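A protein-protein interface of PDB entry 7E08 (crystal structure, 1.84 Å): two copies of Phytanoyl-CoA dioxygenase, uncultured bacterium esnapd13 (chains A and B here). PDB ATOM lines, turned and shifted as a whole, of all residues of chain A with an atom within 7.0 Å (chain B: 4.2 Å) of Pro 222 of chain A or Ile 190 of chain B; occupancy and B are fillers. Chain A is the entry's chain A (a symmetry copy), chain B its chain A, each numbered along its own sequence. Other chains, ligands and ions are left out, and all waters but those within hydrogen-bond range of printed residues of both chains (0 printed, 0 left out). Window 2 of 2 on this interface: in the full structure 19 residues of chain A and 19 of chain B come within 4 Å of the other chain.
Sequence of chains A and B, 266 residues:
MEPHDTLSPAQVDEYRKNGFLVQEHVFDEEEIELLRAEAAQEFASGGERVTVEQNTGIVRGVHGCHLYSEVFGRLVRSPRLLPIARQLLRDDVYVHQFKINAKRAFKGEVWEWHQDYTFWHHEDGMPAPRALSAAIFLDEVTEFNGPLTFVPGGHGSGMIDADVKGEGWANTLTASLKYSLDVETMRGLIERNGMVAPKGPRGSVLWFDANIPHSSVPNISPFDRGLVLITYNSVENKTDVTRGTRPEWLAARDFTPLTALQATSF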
ATOM      1  N   ARG A 104      26.117   6.406  15.767  1.00  0.00           N
ATOM      2  CA  ARG A 104      25.245   5.906  14.712  1.00  0.00           C
ATOM      3  C   ARG A 104      26.089   5.300  13.574  1.00  0.00           C
ATOM      4  O   ARG A 104      27.266   5.655  13.438  1.00  0.00           O
ATOM      5  CB  ARG A 104      24.380   7.052  14.157  1.00  0.00           C
ATOM      6  CG  ARG A 104      23.958   8.148  15.147  1.00  0.00           C
ATOM      7  CD  ARG A 104      23.271   7.669  16.433  1.00  0.00           C
ATOM      8  NE  ARG A 104      22.131   8.546  16.784  1.00  0.00           N
ATOM      9  CZ  ARG A 104      21.206   8.292  17.719  1.00  0.00           C
ATOM     10  NH1 ARG A 104      21.265   7.187  18.461  1.00  0.00           N
ATOM     11  NH2 ARG A 104      20.206   9.156  17.923  1.00  0.00           N
ATOM     12  N   ALA A 105      25.488   4.383  12.811  1.00  0.00           N
ATOM     13  CA  ALA A 105      26.091   3.746  11.630  1.00  0.00           C
ATOM     14  C   ALA A 105      26.847   4.833  10.835  1.00  0.00           C
ATOM     15  O   ALA A 105      26.421   6.028  10.861  1.00  0.00           O
ATOM     16  CB  ALA A 105      24.989   3.107  10.802  1.00  0.00           C
ATOM     17  N   PHE A 106      28.021   4.504  10.263  1.00  0.00           N
ATOM     18  CA  PHE A 106      28.782   5.524   9.449  1.00  0.00           C
ATOM     19  C   PHE A 106      29.062   6.848  10.079  1.00  0.00           C
ATOM     20  O   PHE A 106      29.584   7.767   9.412  1.00  0.00           O
ATOM     21  CB  PHE A 106      28.066   5.840   8.104  1.00  0.00           C
ATOM     22  CG  PHE A 106      27.682   4.626   7.371  1.00  0.00           C
ATOM     23  CD1 PHE A 106      28.656   3.740   6.972  1.00  0.00           C
ATOM     24  CD2 PHE A 106      26.329   4.315   7.144  1.00  0.00           C
ATOM     25  CE1 PHE A 106      28.335   2.565   6.305  1.00  0.00           C
ATOM     26  CE2 PHE A 106      25.989   3.137   6.483  1.00  0.00           C
ATOM     27  CZ  PHE A 106      26.999   2.264   6.051  1.00  0.00           C
ATOM     28  N   PHE A 144      33.872  -3.010  14.293  1.00  0.00           N
ATOM     29  CA  PHE A 144      33.704  -1.972  13.331  1.00  0.00           C
ATOM     30  C   PHE A 144      32.755  -0.887  13.656  1.00  0.00           C
ATOM     31  O   PHE A 144      32.627   0.042  12.907  1.00  0.00           O
ATOM     32  CB  PHE A 144      33.308  -2.637  11.953  1.00  0.00           C
ATOM     33  CG  PHE A 144      34.103  -3.838  11.629  1.00  0.00           C
ATOM     34  CD1 PHE A 144      35.393  -3.674  11.162  1.00  0.00           C
ATOM     35  CD2 PHE A 144      33.589  -5.084  11.726  1.00  0.00           C
ATOM     36  CE1 PHE A 144      36.175  -4.768  10.875  1.00  0.00           C
ATOM     37  CE2 PHE A 144      34.367  -6.200  11.482  1.00  0.00           C
ATOM     38  CZ  PHE A 144      35.683  -6.016  11.042  1.00  0.00           C
ATOM     39  N   ASN A 219      32.423   4.586  13.881  1.00  0.00           N
ATOM     40  CA  ASN A 219      31.572   3.438  13.412  1.00  0.00           C
ATOM     41  C   ASN A 219      31.502   3.504  11.873  1.00  0.00           C
ATOM     42  O   ASN A 219      30.842   4.398  11.306  1.00  0.00           O
ATOM     43  CB  ASN A 219      30.168   3.591  13.973  1.00  0.00           C
ATOM     44  CG  ASN A 219      29.225   2.489  13.612  1.00  0.00           C
ATOM     45  OD1 ASN A 219      29.460   1.600  12.730  1.00  0.00           O
ATOM     46  ND2 ASN A 219      28.050   2.515  14.320  1.00  0.00           N
ATOM     47  N   ILE A 220      32.156   2.547  11.206  1.00  0.00           N
ATOM     48  CA  ILE A 220      32.118   2.487   9.708  1.00  0.00           C
ATOM     49  C   ILE A 220      31.124   1.406   9.289  1.00  0.00           C
ATOM     50  O   ILE A 220      31.034   0.998   8.085  1.00  0.00           O
ATOM     51  CB  ILE A 220      33.541   2.239   9.105  1.00  0.00           C
ATOM     52  CG1 ILE A 220      34.203   1.011   9.764  1.00  0.00           C
ATOM     53  CG2 ILE A 220      34.364   3.522   9.218  1.00  0.00           C
ATOM     54  CD1 ILE A 220      35.195   0.237   8.903  1.00  0.00           C
ATOM     55  N   SER A 221      30.370   0.907  10.266  1.00  0.00           N
ATOM     56  CA  SER A 221      29.445  -0.124   9.995  1.00  0.00           C
ATOM     57  C   SER A 221      28.151   0.643   9.575  1.00  0.00           C
ATOM     58  O   SER A 221      28.065   1.892   9.760  1.00  0.00           O
ATOM     59  CB  SER A 221      29.311  -1.086  11.174  1.00  0.00           C
ATOM     60  OG  SER A 221      28.312  -0.664  12.083  1.00  0.00           O
ATOM     61  N   PRO A 222      27.209  -0.083   8.947  1.00  0.00           N
ATOM     62  CA  PRO A 222      25.833   0.402   8.753  1.00  0.00           C
ATOM     63  C   PRO A 222      24.938   0.199  10.019  1.00  0.00           C
ATOM     64  O   PRO A 222      23.711   0.364   9.919  1.00  0.00           O
ATOM     65  CB  PRO A 222      25.332  -0.463   7.600  1.00  0.00           C
ATOM     66  CG  PRO A 222      26.053  -1.780   7.759  1.00  0.00           C
ATOM     67  CD  PRO A 222      27.329  -1.503   8.529  1.00  0.00           C
ATOM     68  N   PHE A 223      25.545  -0.084  11.185  1.00  0.00           N
ATOM     69  CA  PHE A 223      24.803  -0.357  12.417  1.00  0.00           C
ATOM     70  C   PHE A 223      25.211   0.574  13.574  1.00  0.00           C
ATOM     71  O   PHE A 223      26.378   0.843  13.764  1.00  0.00           O
ATOM     72  CB  PHE A 223      25.062  -1.771  12.846  1.00  0.00           C
ATOM     73  CG  PHE A 223      24.861  -2.784  11.758  1.00  0.00           C
ATOM     74  CD1 PHE A 223      23.617  -2.927  11.149  1.00  0.00           C
ATOM     75  CD2 PHE A 223      25.910  -3.628  11.368  1.00  0.00           C
ATOM     76  CE1 PHE A 223      23.419  -3.876  10.169  1.00  0.00           C
ATOM     77  CE2 PHE A 223      25.715  -4.574  10.387  1.00  0.00           C
ATOM     78  CZ  PHE A 223      24.466  -4.703   9.792  1.00  0.00           C
ATOM     79  N   ASP A 224      24.248   0.997  14.400  1.00  0.00           N
ATOM     80  CA  ASP A 224      24.532   1.891  15.514  1.00  0.00           C
ATOM     81  C   ASP A 224      25.309   1.228  16.643  1.00  0.00           C
ATOM     82  O   ASP A 224      25.317   0.028  16.781  1.00  0.00           O
ATOM     83  CB  ASP A 224      23.196   2.451  16.072  1.00  0.00           C
ATOM     84  CG  ASP A 224      22.434   3.276  15.013  1.00  0.00           C
ATOM     85  OD1 ASP A 224      22.963   3.396  13.892  1.00  0.00           O
ATOM     86  OD2 ASP A 224      21.321   3.764  15.261  1.00  0.00           O
ATOM     87  N   VAL B 151      34.364  -5.910   2.645  1.00  0.00           N
ATOM     88  CA  VAL B 151      33.216  -6.869   2.609  1.00  0.00           C
ATOM     89  C   VAL B 151      33.568  -8.151   1.877  1.00  0.00           C
ATOM     90  O   VAL B 151      33.667  -8.092   0.691  1.00  0.00           O
ATOM     91  CB  VAL B 151      32.077  -6.195   1.808  1.00  0.00           C
ATOM     92  CG1 VAL B 151      30.842  -7.125   1.754  1.00  0.00           C
ATOM     93  CG2 VAL B 151      31.768  -4.784   2.283  1.00  0.00           C
ATOM     94  N   MET B 186      25.696  -0.070   1.376  1.00  0.00           N
ATOM     95  CA  MET B 186      26.545  -0.753   2.330  1.00  0.00           C
ATOM     96  C   MET B 186      25.823  -1.641   3.328  1.00  0.00           C
ATOM     97  O   MET B 186      26.304  -2.719   3.630  1.00  0.00           O
ATOM     98  CB  MET B 186      27.438   0.232   3.013  1.00  0.00           C
ATOM     99  CG  MET B 186      28.424   0.927   2.074  1.00  0.00           C
ATOM    100  SD  MET B 186      29.597  -0.141   1.202  1.00  0.00           S
ATOM    101  CE  MET B 186      29.726  -1.542   2.261  1.00  0.00           C
ATOM    102  N   ARG B 187      24.650  -1.208   3.816  1.00  0.00           N
ATOM    103  CA  ARG B 187      23.926  -2.004   4.753  1.00  0.00           C
ATOM    104  C   ARG B 187      23.623  -3.354   4.219  1.00  0.00           C
ATOM    105  O   ARG B 187      23.870  -4.369   4.910  1.00  0.00           O
ATOM    106  CB  ARG B 187      22.637  -1.275   5.217  1.00  0.00           C
ATOM    107  CG  ARG B 187      21.960  -1.981   6.407  1.00  0.00           C
ATOM    108  CD  ARG B 187      20.675  -1.333   6.916  1.00  0.00           C
ATOM    109  NE  ARG B 187      20.432   0.004   6.380  1.00  0.00           N
ATOM    110  CZ  ARG B 187      20.915   1.154   6.869  1.00  0.00           C
ATOM    111  NH1 ARG B 187      21.728   1.214   7.946  1.00  0.00           N
ATOM    112  NH2 ARG B 187      20.582   2.278   6.243  1.00  0.00           N
ATOM    113  N   GLY B 188      23.119  -3.434   2.960  1.00  0.00           N
ATOM    114  CA  GLY B 188      22.726  -4.759   2.414  1.00  0.00           C
ATOM    115  C   GLY B 188      23.900  -5.704   2.234  1.00  0.00           C
ATOM    116  O   GLY B 188      23.865  -6.948   2.597  1.00  0.00           O
ATOM    117  N   LEU B 189      24.958  -5.095   1.668  1.00  0.00           N
ATOM    118  CA  LEU B 189      26.275  -5.754   1.486  1.00  0.00           C
ATOM    119  C   LEU B 189      26.679  -6.439   2.783  1.00  0.00           C
ATOM    120  O   LEU B 189      26.816  -7.699   2.915  1.00  0.00           O
ATOM    121  CB  LEU B 189      27.307  -4.707   1.040  1.00  0.00           C
ATOM    122  CG  LEU B 189      27.867  -4.681  -0.420  1.00  0.00           C
ATOM    123  CD1 LEU B 189      27.046  -5.460  -1.428  1.00  0.00           C
ATOM    124  CD2 LEU B 189      28.137  -3.267  -0.936  1.00  0.00           C
ATOM    125  N   ILE B 190      26.711  -5.609   3.808  1.00  0.00           N
ATOM    126  CA  ILE B 190      27.187  -6.092   5.092  1.00  0.00           C
ATOM    127  C   ILE B 190      26.232  -7.002   5.766  1.00  0.00           C
ATOM    128  O   ILE B 190      26.681  -7.976   6.379  1.00  0.00           O
ATOM    129  CB  ILE B 190      27.688  -4.949   5.965  1.00  0.00           C
ATOM    130  CG1 ILE B 190      28.904  -4.327   5.267  1.00  0.00           C
ATOM    131  CG2 ILE B 190      28.053  -5.458   7.368  1.00  0.00           C
ATOM    132  CD1 ILE B 190      29.088  -2.835   5.540  1.00  0.00           C
ATOM    133  N   GLU B 191      24.905  -6.827   5.598  1.00  0.00           N
ATOM    134  CA  GLU B 191      24.019  -7.847   6.170  1.00  0.00           C
ATOM    135  C   GLU B 191      24.219  -9.146   5.520  1.00  0.00           C
ATOM    136  O   GLU B 191      24.168 -10.199   6.171  1.00  0.00           O
ATOM    137  CB  GLU B 191      22.567  -7.429   6.045  1.00  0.00           C
ATOM    138  CG  GLU B 191      22.229  -6.257   6.966  1.00  0.00           C
ATOM    139  CD  GLU B 191      20.889  -5.600   6.651  1.00  0.00           C
ATOM    140  OE1 GLU B 191      20.377  -5.744   5.495  1.00  0.00           O
ATOM    141  OE2 GLU B 191      20.374  -4.917   7.576  1.00  0.00           O
ATOM    142  N   ARG B 192      24.464  -9.082   4.207  1.00  0.00           N
ATOM    143  CA  ARG B 192      24.615 -10.300   3.410  1.00  0.00           C
ATOM    144  C   ARG B 192      25.939 -10.986   3.744  1.00  0.00           C
ATOM    145  O   ARG B 192      26.003 -12.239   3.959  1.00  0.00           O
ATOM    146  CB  ARG B 192      24.483  -9.975   1.908  1.00  0.00           C
ATOM    147  CG  ARG B 192      23.056  -9.665   1.401  1.00  0.00           C
ATOM    148  CD  ARG B 192      22.959  -9.528  -0.125  1.00  0.00           C
ATOM    149  NE  ARG B 192      23.405  -8.228  -0.675  1.00  0.00           N
ATOM    150  CZ  ARG B 192      22.704  -7.093  -0.674  1.00  0.00           C
ATOM    151  NH1 ARG B 192      21.485  -7.061  -0.141  1.00  0.00           N
ATOM    152  NH2 ARG B 192      23.222  -5.965  -1.204  1.00  0.00           N
ATOM    153  N   ASN B 193      26.990 -10.160   3.867  1.00  0.00           N
ATOM    154  CA  ASN B 193      28.363 -10.705   3.790  1.00  0.00           C
ATOM    155  C   ASN B 193      29.303 -10.520   5.009  1.00  0.00           C
ATOM    156  O   ASN B 193      30.305 -11.255   5.154  1.00  0.00           O
ATOM    157  CB  ASN B 193      28.984 -10.077   2.553  1.00  0.00           C
ATOM    158  CG  ASN B 193      28.223 -10.429   1.301  1.00  0.00           C
ATOM    159  OD1 ASN B 193      28.107 -11.599   1.017  1.00  0.00           O
ATOM    160  ND2 ASN B 193      27.681  -9.426   0.571  1.00  0.00           N
ATOM    161  N   GLY B 194      28.989  -9.528   5.835  1.00  0.00           N
ATOM    162  CA  GLY B 194      29.826  -9.137   6.977  1.00  0.00           C
ATOM    163  C   GLY B 194      31.006  -8.227   6.559  1.00  0.00           C
ATOM    164  O   GLY B 194      30.996  -7.605   5.469  1.00  0.00           O
ATOM    165  N   MET B 195      31.954  -8.090   7.501  1.00  0.00           N
ATOM    166  CA  MET B 195      33.166  -7.210   7.391  1.00  0.00           C
ATOM    167  C   MET B 195      34.306  -7.957   8.005  1.00  0.00           C
ATOM    168  O   MET B 195      34.152  -8.716   9.024  1.00  0.00           O
ATOM    169  CB  MET B 195      33.063  -5.892   8.083  1.00  0.00           C
ATOM    170  CG  MET B 195      32.205  -4.824   7.443  1.00  0.00           C
ATOM    171  SD  MET B 195      31.636  -3.586   8.701  1.00  0.00           S
ATOM    172  CE  MET B 195      30.767  -4.765   9.695  1.00  0.00           C
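Hydrophobic or aromatic side chains of chain A within 4 Å of the printed part of chain B: Phe 106, Phe 144, Pro 222 and Phe 223. Along chain A the printed residues that touch a printed residue of chain B span positions 106 to 223. Of the 11 printed residues of chain B, 5 touch a printed residue of chain A. Among the printed residues, 6 pairs touch across the chains. Among the printed residues, no Asp or Glu carboxylate lies within 4 Å of a Lys or Arg side-chain nitrogen of the other chain.
Among the printed residues, pairs that only touch across the chains: Phe 144 of chain A with Met 195 of chain B (3.5 Å), Phe 106 of chain A with Met 186 of chain B (3.7 Å), Pro 222 of chain A with Ile 190 of chain B (3.7 Å), Phe 223 of chain A with Ile 190 of chain B (3.9 Å) and Phe 223 of chain A with Glu 191 of chain B (3.9 Å).
O of Pro 222 of chain A is in hydrogen-bond range of NH1 of Arg 187 of chain B (2.9 Å).
Printed residues of chain B within 4 Å of Phe 144 of chain A: Met 195. Ile 220 of chain A touches none of the printed residues of chain B. Of chain B, only Arg 187 and Ile 190 come within 4 Å of Pro 222 of chain A. Of the printed residues of chain A, Met 186 of chain B touches Phe 106. Of chain A, only Pro 222 and Phe 223 come within 4 Å of Ile 190 of chain B.
O of Ser 221 of chain A lies within hydrogen-bond range of N of Phe 106 of chain A, 2.7 Å away. The backbone NH (N) of Phe 106 of chain A lies close to the backbone carbonyl oxygen (O) of Asn 219 of chain A. The side-chain amide nitrogen (ND2) of Asn 219 of chain A lies within hydrogen-bond range of the backbone carbonyl oxygen (O) of Phe 223 of chain A (2.4 Å). The backbone NH (N) of Phe 223 of chain A lies within hydrogen-bond range of the side-chain hydroxyl (OG) of Ser 221 of chain A, at 3.0 Å. The backbone NH of Ile 220 of chain A lies within hydrogen-bond range of the backbone carbonyl oxygen of Phe 144 of chain A, 3.1 Å away.
No position is printed for both chains. Of the 6 pairs that touch across the chains among the printed residues, none has its exchanged pair printed and touching as well.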
